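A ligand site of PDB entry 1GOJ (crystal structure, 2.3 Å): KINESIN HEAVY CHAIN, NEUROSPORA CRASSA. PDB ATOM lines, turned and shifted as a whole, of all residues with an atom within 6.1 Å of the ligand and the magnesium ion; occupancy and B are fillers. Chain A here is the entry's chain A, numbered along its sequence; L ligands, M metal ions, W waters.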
ATOM      1  N   ARG A  13     -13.346 -21.573  27.883  1.00  0.00           N
ATOM      2  CA  ARG A  13     -13.363 -22.026  26.503  1.00  0.00           C
ATOM      3  C   ARG A  13     -14.074 -23.368  26.387  1.00  0.00           C
ATOM      4  O   ARG A  13     -13.669 -24.355  26.999  1.00  0.00           O
ATOM      5  CB  ARG A  13     -11.947 -22.185  25.937  1.00  0.00           C
ATOM      6  CG  ARG A  13     -11.989 -22.670  24.472  1.00  0.00           C
ATOM      7  CD  ARG A  13     -10.629 -22.956  23.874  1.00  0.00           C
ATOM      8  NE  ARG A  13     -10.738 -23.029  22.417  1.00  0.00           N
ATOM      9  CZ  ARG A  13      -9.748 -23.344  21.585  1.00  0.00           C
ATOM     10  NH1 ARG A  13      -8.544 -23.633  22.062  1.00  0.00           N
ATOM     11  NH2 ARG A  13      -9.960 -23.357  20.281  1.00  0.00           N
ATOM     12  N   PHE A  14     -15.150 -23.385  25.597  1.00  0.00           N
ATOM     13  CA  PHE A  14     -15.919 -24.594  25.369  1.00  0.00           C
ATOM     14  C   PHE A  14     -15.529 -25.154  24.007  1.00  0.00           C
ATOM     15  O   PHE A  14     -15.577 -24.440  23.001  1.00  0.00           O
ATOM     16  CB  PHE A  14     -17.421 -24.292  25.377  1.00  0.00           C
ATOM     17  CG  PHE A  14     -17.987 -24.000  26.744  1.00  0.00           C
ATOM     18  CD1 PHE A  14     -18.601 -25.007  27.488  1.00  0.00           C
ATOM     19  CD2 PHE A  14     -17.889 -22.725  27.301  1.00  0.00           C
ATOM     20  CE1 PHE A  14     -19.105 -24.743  28.763  1.00  0.00           C
ATOM     21  CE2 PHE A  14     -18.386 -22.452  28.569  1.00  0.00           C
ATOM     22  CZ  PHE A  14     -18.994 -23.465  29.310  1.00  0.00           C
ATOM     23  N   ARG A  15     -15.162 -26.422  23.990  1.00  0.00           N
ATOM     24  CA  ARG A  15     -14.803 -27.096  22.749  1.00  0.00           C
ATOM     25  C   ARG A  15     -16.052 -27.807  22.241  1.00  0.00           C
ATOM     26  O   ARG A  15     -17.043 -27.929  22.951  1.00  0.00           O
ATOM     27  CB  ARG A  15     -13.739 -28.179  23.018  1.00  0.00           C
ATOM     28  CG  ARG A  15     -14.211 -29.256  24.020  1.00  0.00           C
ATOM     29  CD  ARG A  15     -13.446 -30.566  23.820  1.00  0.00           C
ATOM     30  NE  ARG A  15     -13.702 -31.561  24.867  1.00  0.00           N
ATOM     31  CZ  ARG A  15     -14.873 -32.152  25.097  1.00  0.00           C
ATOM     32  NH1 ARG A  15     -15.942 -31.860  24.365  1.00  0.00           N
ATOM     33  NH2 ARG A  15     -14.965 -33.065  26.054  1.00  0.00           N
ATOM     34  N   PRO A  16     -16.026 -28.255  20.977  1.00  0.00           N
ATOM     35  CA  PRO A  16     -17.179 -28.970  20.412  1.00  0.00           C
ATOM     36  C   PRO A  16     -17.270 -30.315  21.158  1.00  0.00           C
ATOM     37  O   PRO A  16     -16.288 -30.749  21.760  1.00  0.00           O
ATOM     38  CB  PRO A  16     -16.778 -29.186  18.957  1.00  0.00           C
ATOM     39  CG  PRO A  16     -15.894 -27.998  18.671  1.00  0.00           C
ATOM     40  CD  PRO A  16     -15.062 -27.890  19.931  1.00  0.00           C
ATOM     41  N   MET A  57     -17.962 -22.868  21.176  1.00  0.00           N
ATOM     42  CA  MET A  57     -17.462 -23.967  20.349  1.00  0.00           C
ATOM     43  C   MET A  57     -16.908 -23.579  18.982  1.00  0.00           C
ATOM     44  O   MET A  57     -16.119 -24.330  18.394  1.00  0.00           O
ATOM     45  CB  MET A  57     -18.549 -25.016  20.141  1.00  0.00           C
ATOM     46  CG  MET A  57     -19.043 -25.675  21.403  1.00  0.00           C
ATOM     47  SD  MET A  57     -20.102 -24.611  22.417  1.00  0.00           S
ATOM     48  CE  MET A  57     -21.704 -24.879  21.614  1.00  0.00           C
ATOM     49  N   CYS A  59     -15.139 -20.691  18.324  1.00  0.00           N
ATOM     50  CA  CYS A  59     -13.882 -19.956  18.440  1.00  0.00           C
ATOM     51  C   CYS A  59     -12.643 -20.761  18.078  1.00  0.00           C
ATOM     52  O   CYS A  59     -12.453 -21.884  18.561  1.00  0.00           O
ATOM     53  CB  CYS A  59     -13.758 -19.373  19.843  1.00  0.00           C
ATOM     54  SG  CYS A  59     -15.074 -18.184  20.221  1.00  0.00           S
ATOM     55  N   GLN A  61      -8.244 -21.124  17.351  1.00  0.00           N
ATOM     56  CA  GLN A  61      -7.000 -20.865  18.066  1.00  0.00           C
ATOM     57  C   GLN A  61      -6.564 -19.407  17.978  1.00  0.00           C
ATOM     58  O   GLN A  61      -6.117 -18.842  18.973  1.00  0.00           O
ATOM     59  CB  GLN A  61      -5.895 -21.776  17.535  1.00  0.00           C
ATOM     60  CG  GLN A  61      -6.235 -23.270  17.628  1.00  0.00           C
ATOM     61  CD  GLN A  61      -6.061 -23.832  19.028  1.00  0.00           C
ATOM     62  OE1 GLN A  61      -5.303 -24.787  19.235  1.00  0.00           O
ATOM     63  NE2 GLN A  61      -6.768 -23.261  19.997  1.00  0.00           N
ATOM     64  N   GLY A  88      -8.893 -27.903  33.580  1.00  0.00           N
ATOM     65  CA  GLY A  88     -10.075 -28.629  33.155  1.00  0.00           C
ATOM     66  C   GLY A  88      -9.927 -30.137  33.181  1.00  0.00           C
ATOM     67  O   GLY A  88      -8.832 -30.668  33.306  1.00  0.00           O
ATOM     68  N   GLN A  89     -11.045 -30.843  33.037  1.00  0.00           N
ATOM     69  CA  GLN A  89     -11.041 -32.300  33.063  1.00  0.00           C
ATOM     70  C   GLN A  89     -10.292 -32.876  31.868  1.00  0.00           C
ATOM     71  O   GLN A  89     -10.113 -32.219  30.847  1.00  0.00           O
ATOM     72  CB  GLN A  89     -12.487 -32.829  33.084  1.00  0.00           C
ATOM     73  CG  GLN A  89     -13.034 -33.234  31.720  1.00  0.00           C
ATOM     74  CD  GLN A  89     -14.511 -33.577  31.735  1.00  0.00           C
ATOM     75  OE1 GLN A  89     -15.364 -32.695  31.546  1.00  0.00           O
ATOM     76  NE2 GLN A  89     -14.829 -34.844  31.990  1.00  0.00           N
ATOM     77  N   THR A  90      -9.833 -34.117  32.001  1.00  0.00           N
ATOM     78  CA  THR A  90      -9.126 -34.782  30.917  1.00  0.00           C
ATOM     79  C   THR A  90     -10.034 -34.786  29.686  1.00  0.00           C
ATOM     80  O   THR A  90     -11.235 -35.049  29.791  1.00  0.00           O
ATOM     81  CB  THR A  90      -8.738 -36.228  31.315  1.00  0.00           C
ATOM     82  OG1 THR A  90      -7.768 -36.174  32.381  1.00  0.00           O
ATOM     83  CG2 THR A  90      -8.115 -36.978  30.129  1.00  0.00           C
ATOM     84  N   GLY A  91      -9.457 -34.471  28.530  1.00  0.00           N
ATOM     85  CA  GLY A  91     -10.227 -34.424  27.306  1.00  0.00           C
ATOM     86  C   GLY A  91     -10.938 -33.097  27.066  1.00  0.00           C
ATOM     87  O   GLY A  91     -11.616 -32.943  26.055  1.00  0.00           O
ATOM     88  N   ALA A  92     -10.802 -32.135  27.979  1.00  0.00           N
ATOM     89  CA  ALA A  92     -11.469 -30.839  27.814  1.00  0.00           C
ATOM     90  C   ALA A  92     -10.794 -29.895  26.826  1.00  0.00           C
ATOM     91  O   ALA A  92     -11.450 -29.020  26.254  1.00  0.00           O
ATOM     92  CB  ALA A  92     -11.618 -30.149  29.168  1.00  0.00           C
ATOM     93  N   GLY A  93      -9.493 -30.058  26.604  1.00  0.00           N
ATOM     94  CA  GLY A  93      -8.808 -29.205  25.648  1.00  0.00           C
ATOM     95  C   GLY A  93      -7.680 -28.355  26.180  1.00  0.00           C
ATOM     96  O   GLY A  93      -7.370 -27.297  25.616  1.00  0.00           O
ATOM     97  N   LYS A  94      -7.042 -28.799  27.266  1.00  0.00           N
ATOM     98  CA  LYS A  94      -5.926 -28.053  27.847  1.00  0.00           C
ATOM     99  C   LYS A  94      -4.704 -28.025  26.924  1.00  0.00           C
ATOM    100  O   LYS A  94      -4.184 -26.957  26.593  1.00  0.00           O
ATOM    101  CB  LYS A  94      -5.542 -28.633  29.208  1.00  0.00           C
ATOM    102  CG  LYS A  94      -6.631 -28.496  30.262  1.00  0.00           C
ATOM    103  CD  LYS A  94      -6.187 -29.095  31.592  1.00  0.00           C
ATOM    104  CE  LYS A  94      -5.830 -30.569  31.447  1.00  0.00           C
ATOM    105  NZ  LYS A  94      -6.991 -31.418  31.082  1.00  0.00           N
ATOM    106  N   SER A  95      -4.250 -29.211  26.501  1.00  0.00           N
ATOM    107  CA  SER A  95      -3.081 -29.312  25.612  1.00  0.00           C
ATOM    108  C   SER A  95      -3.370 -28.718  24.238  1.00  0.00           C
ATOM    109  O   SER A  95      -2.521 -28.060  23.633  1.00  0.00           O
ATOM    110  CB  SER A  95      -2.654 -30.787  25.445  1.00  0.00           C
ATOM    111  OG  SER A  95      -2.341 -31.368  26.692  1.00  0.00           O
ATOM    112  N   TYR A  96      -4.578 -28.964  23.721  1.00  0.00           N
ATOM    113  CA  TYR A  96      -4.966 -28.433  22.425  1.00  0.00           C
ATOM    114  C   TYR A  96      -4.877 -26.908  22.469  1.00  0.00           C
ATOM    115  O   TYR A  96      -4.425 -26.274  21.520  1.00  0.00           O
ATOM    116  CB  TYR A  96      -6.395 -28.840  22.093  1.00  0.00           C
ATOM    117  CG  TYR A  96      -6.903 -28.251  20.791  1.00  0.00           C
ATOM    118  CD1 TYR A  96      -6.649 -28.871  19.577  1.00  0.00           C
ATOM    119  CD2 TYR A  96      -7.603 -27.046  20.782  1.00  0.00           C
ATOM    120  CE1 TYR A  96      -7.084 -28.314  18.372  1.00  0.00           C
ATOM    121  CE2 TYR A  96      -8.044 -26.482  19.581  1.00  0.00           C
ATOM    122  CZ  TYR A  96      -7.785 -27.118  18.381  1.00  0.00           C
ATOM    123  OH  TYR A  96      -8.226 -26.563  17.197  1.00  0.00           O
ATOM    124  N   THR A  97      -5.308 -26.320  23.574  1.00  0.00           N
ATOM    125  CA  THR A  97      -5.287 -24.863  23.728  1.00  0.00           C
ATOM    126  C   THR A  97      -3.872 -24.308  23.934  1.00  0.00           C
ATOM    127  O   THR A  97      -3.526 -23.258  23.388  1.00  0.00           O
ATOM    128  CB  THR A  97      -6.155 -24.417  24.934  1.00  0.00           C
ATOM    129  OG1 THR A  97      -7.523 -24.799  24.705  1.00  0.00           O
ATOM    130  CG2 THR A  97      -6.089 -22.918  25.132  1.00  0.00           C
ATOM    131  N   THR A 101      -2.958 -29.160  18.225  1.00  0.00           N
ATOM    132  CA  THR A 101      -2.930 -30.485  17.612  1.00  0.00           C
ATOM    133  C   THR A 101      -1.510 -30.815  17.171  1.00  0.00           C
ATOM    134  O   THR A 101      -0.985 -31.908  17.416  1.00  0.00           O
ATOM    135  CB  THR A 101      -3.877 -30.512  16.391  1.00  0.00           C
ATOM    136  OG1 THR A 101      -3.881 -31.822  15.807  1.00  0.00           O
ATOM    137  CG2 THR A 101      -3.443 -29.488  15.350  1.00  0.00           C
ATOM    138  N   ARG A 194       7.738 -36.168  26.648  1.00  0.00           N
ATOM    139  CA  ARG A 194       6.516 -36.452  27.395  1.00  0.00           C
ATOM    140  C   ARG A 194       5.869 -37.785  27.003  1.00  0.00           C
ATOM    141  O   ARG A 194       5.336 -38.492  27.857  1.00  0.00           O
ATOM    142  CB  ARG A 194       5.482 -35.339  27.198  1.00  0.00           C
ATOM    143  CG  ARG A 194       5.849 -33.993  27.772  1.00  0.00           C
ATOM    144  CD  ARG A 194       4.731 -33.397  28.635  1.00  0.00           C
ATOM    145  NE  ARG A 194       3.641 -32.841  27.836  1.00  0.00           N
ATOM    146  CZ  ARG A 194       2.459 -32.481  28.352  1.00  0.00           C
ATOM    147  NH1 ARG A 194       2.225 -32.618  29.650  1.00  0.00           N
ATOM    148  NH2 ARG A 194       1.519 -31.975  27.563  1.00  0.00           N
ATOM    149  N   SER A 205      -0.601 -39.924  31.833  1.00  0.00           N
ATOM    150  CA  SER A 205      -0.391 -38.636  31.171  1.00  0.00           C
ATOM    151  C   SER A 205      -1.400 -37.570  31.602  1.00  0.00           C
ATOM    152  O   SER A 205      -1.106 -36.372  31.582  1.00  0.00           O
ATOM    153  CB  SER A 205      -0.472 -38.835  29.650  1.00  0.00           C
ATOM    154  OG  SER A 205      -0.164 -37.643  28.952  1.00  0.00           O
ATOM    155  N   ASP A 235       0.177 -26.476  31.517  1.00  0.00           N
ATOM    156  CA  ASP A 235      -0.840 -27.429  31.068  1.00  0.00           C
ATOM    157  C   ASP A 235      -1.025 -28.347  32.269  1.00  0.00           C
ATOM    158  O   ASP A 235      -0.241 -29.274  32.490  1.00  0.00           O
ATOM    159  CB  ASP A 235      -0.323 -28.219  29.871  1.00  0.00           C
ATOM    160  CG  ASP A 235      -1.375 -29.158  29.282  1.00  0.00           C
ATOM    161  OD1 ASP A 235      -2.407 -29.391  29.957  1.00  0.00           O
ATOM    162  OD2 ASP A 235      -1.163 -29.669  28.168  1.00  0.00           O
ATOM    163  N   LEU A 236      -2.068 -28.079  33.054  1.00  0.00           N
ATOM    164  CA  LEU A 236      -2.338 -28.848  34.263  1.00  0.00           C
ATOM    165  C   LEU A 236      -2.855 -30.258  34.069  1.00  0.00           C
ATOM    166  O   LEU A 236      -3.378 -30.624  32.996  1.00  0.00           O
ATOM    167  CB  LEU A 236      -3.343 -28.083  35.135  1.00  0.00           C
ATOM    168  CG  LEU A 236      -2.973 -26.675  35.618  1.00  0.00           C
ATOM    169  CD1 LEU A 236      -4.220 -26.008  36.189  1.00  0.00           C
ATOM    170  CD2 LEU A 236      -1.885 -26.739  36.670  1.00  0.00           C
ATOM    171  N   ASN A 306     -10.952 -24.956  30.555  1.00  0.00           N
ATOM    172  CA  ASN A 306     -11.451 -25.707  29.408  1.00  0.00           C
ATOM    173  C   ASN A 306     -12.668 -26.531  29.809  1.00  0.00           C
ATOM    174  O   ASN A 306     -12.625 -27.310  30.770  1.00  0.00           O
ATOM    175  CB  ASN A 306     -10.335 -26.587  28.860  1.00  0.00           C
ATOM    176  CG  ASN A 306      -9.228 -25.780  28.234  1.00  0.00           C
ATOM    177  OD1 ASN A 306      -9.371 -25.264  27.114  1.00  0.00           O
ATOM    178  ND2 ASN A 306      -8.109 -25.634  28.945  1.00  0.00           N
HETATM  179  P1  LIG L   1      -6.721 -32.306  27.650  1.00  0.00           P
HETATM  180  O1  LIG L   1      -6.927 -33.749  27.939  1.00  0.00           O
HETATM  181  O2  LIG L   1      -7.451 -31.296  28.450  1.00  0.00           O
HETATM  182  O3  LIG L   1      -5.250 -32.018  27.572  1.00  0.00           O
HETATM  183  P2  LIG L   1      -6.821 -32.319  24.684  1.00  0.00           P
HETATM  184  O4  LIG L   1      -6.502 -30.916  24.353  1.00  0.00           O
HETATM  185  O5  LIG L   1      -5.800 -33.400  24.605  1.00  0.00           O
HETATM  186  O6  LIG L   1      -7.175 -31.908  26.183  1.00  0.00           O
HETATM  187  O7  LIG L   1      -8.174 -32.706  23.913  1.00  0.00           O
HETATM  188  C1  LIG L   1      -8.542 -34.076  23.496  1.00  0.00           C
HETATM  189  C2  LIG L   1      -9.149 -33.904  22.068  1.00  0.00           C
HETATM  190  O8  LIG L   1      -9.634 -32.534  22.022  1.00  0.00           O
HETATM  191  C3  LIG L   1      -8.044 -33.905  21.072  1.00  0.00           C
HETATM  192  O9  LIG L   1      -8.090 -34.951  20.084  1.00  0.00           O
HETATM  193  C4  LIG L   1      -8.136 -32.410  20.692  1.00  0.00           C
HETATM  194  O10 LIG L   1      -7.539 -32.126  19.464  1.00  0.00           O
HETATM  195  C5  LIG L   1      -9.579 -32.069  20.744  1.00  0.00           C
HETATM  196  N1  LIG L   1     -10.004 -30.676  20.914  1.00  0.00           N
HETATM  197  C6  LIG L   1      -9.922 -29.920  22.013  1.00  0.00           C
HETATM  198  N2  LIG L   1     -10.407 -28.693  21.838  1.00  0.00           N
HETATM  199  C7  LIG L   1     -10.780 -28.708  20.610  1.00  0.00           C
HETATM  200  C8  LIG L   1     -11.355 -27.613  20.006  1.00  0.00           C
HETATM  201  N3  LIG L   1     -11.545 -26.469  20.636  1.00  0.00           N
HETATM  202  N4  LIG L   1     -11.691 -27.829  18.686  1.00  0.00           N
HETATM  203  C9  LIG L   1     -11.491 -28.996  18.033  1.00  0.00           C
HETATM  204  N5  LIG L   1     -10.932 -30.056  18.655  1.00  0.00           N
HETATM  205  C10 LIG L   1     -10.563 -29.915  19.982  1.00  0.00           C
HETATM  206 MG    MG M   1      -3.336 -32.970  27.708  1.00  0.00          MG
HETATM  207  O   HOH W   1      -4.427 -32.245  19.563  1.00  0.00           O
HETATM  208  O   HOH W   2      -3.690 -34.031  25.954  1.00  0.00           O
HETATM  209  O   HOH W   3     -10.416 -26.384  23.599  1.00  0.00           O
HETATM  210  O   HOH W   4      -6.776 -35.969  26.643  1.00  0.00           O
HETATM  211  O   HOH W   5      -5.972 -36.061  23.886  1.00  0.00           O
HETATM  212  O   HOH W   6      -4.422 -34.527  28.983  1.00  0.00           O
HETATM  213  O   HOH W   7      -1.812 -33.905  27.981  1.00  0.00           O
HETATM  214  O   HOH W   8      -2.993 -31.900  29.479  1.00  0.00           O
HETATM  215  O   HOH W   9     -12.705 -33.438  21.252  1.00  0.00           O
HETATM  216  O   HOH W  10     -13.462 -24.775  18.768  1.00  0.00           O
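O3 of the ligand sits close to N of Ser 95, 3.2 Å away.
N of Gly 91 sits at hydrogen-bond distance from O1 of the ligand, 2.7 Å away.
An oxygen (O2) of the ligand lies within hydrogen-bond range of the backbone NH (N) of Lys 94 (2.8 Å).
The side-chain amino group (NZ) of Lys 94 is in salt-bridge range of an oxygen (O2) of the ligand, 2.7 Å away.
An oxygen (O4) of the ligand sits at hydrogen-bond distance from the backbone NH of Tyr 96, at 2.8 Å.
The backbone NH (N) of Gly 93 sits at hydrogen-bond distance from an oxygen (O6) of the ligand (3.0 Å).
N of Ala 92 is in hydrogen-bond range of O2 of the ligand (3.5 Å).
The guanidinium group of Arg 13 sits at hydrogen-bond distance from the side-chain hydroxyl of Thr 97 (3.1 Å).
The side-chain amide oxygen (OE1) of Gln 61 sits close to the backbone carbonyl oxygen (O) of Tyr 96 (2.9 Å).
The side-chain amide nitrogen of Gln 61 sits close to the guanidinium group of Arg 13 (2.7 Å).
The side-chain carboxylate (OD2) of Asp 235 sits close to the side-chain hydroxyl (OG) of Ser 95 (2.5 Å).
The backbone carbonyl oxygen of Gly 91 sits at hydrogen-bond distance from the guanidinium group of Arg 15 (2.8 Å).
The backbone carbonyl oxygen of Gly 93 sits at hydrogen-bond distance from the side-chain hydroxyl of Thr 97 (2.7 Å).
The side-chain amino group (NZ) of Lys 94 sits at hydrogen-bond distance from the backbone carbonyl oxygen (O) of Gln 89.
The side-chain amino group (NZ) of Lys 94 sits at hydrogen-bond distance from the backbone carbonyl oxygen (O) of Gly 88 (3.0 Å).
Arg 13 touches the ligand.
Arg 15 touches the ligand (CB to N2, 3.6 Å).
CD of Pro 16 touches N4 of the ligand, at 3.6 Å.
Gln 89 touches the ligand.
Thr 90 touches the ligand (C to O1, 3.7 Å).
Hydrophobic or aromatic side chains within 4 Å of the ligand: Pro 16 and Tyr 96.
Of the 23 residues printed, 11 come within 4 Å of the ligand.
Asp 235 touches the magnesium ion.
Within 4 Å of the magnesium ion: Ser 95 and Asp 235.
The magnesium ion is bound by water W7 (1.8 Å), water W2 (2.1 Å), water W8 (2.1 Å), an oxygen (O3) of the ligand (2.1 Å), the side-chain hydroxyl of Ser 95 (2.1 Å) and water W6 (2.3 Å).
Water W3 lies within hydrogen-bond range of N2 of the ligand and OG1 of Thr 97.
Water W10 lies within hydrogen-bond range of the backbone carbonyl oxygen of Met 57, the backbone carbonyl oxygen of Cys 59 and a nitrogen (N3) of the ligand.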
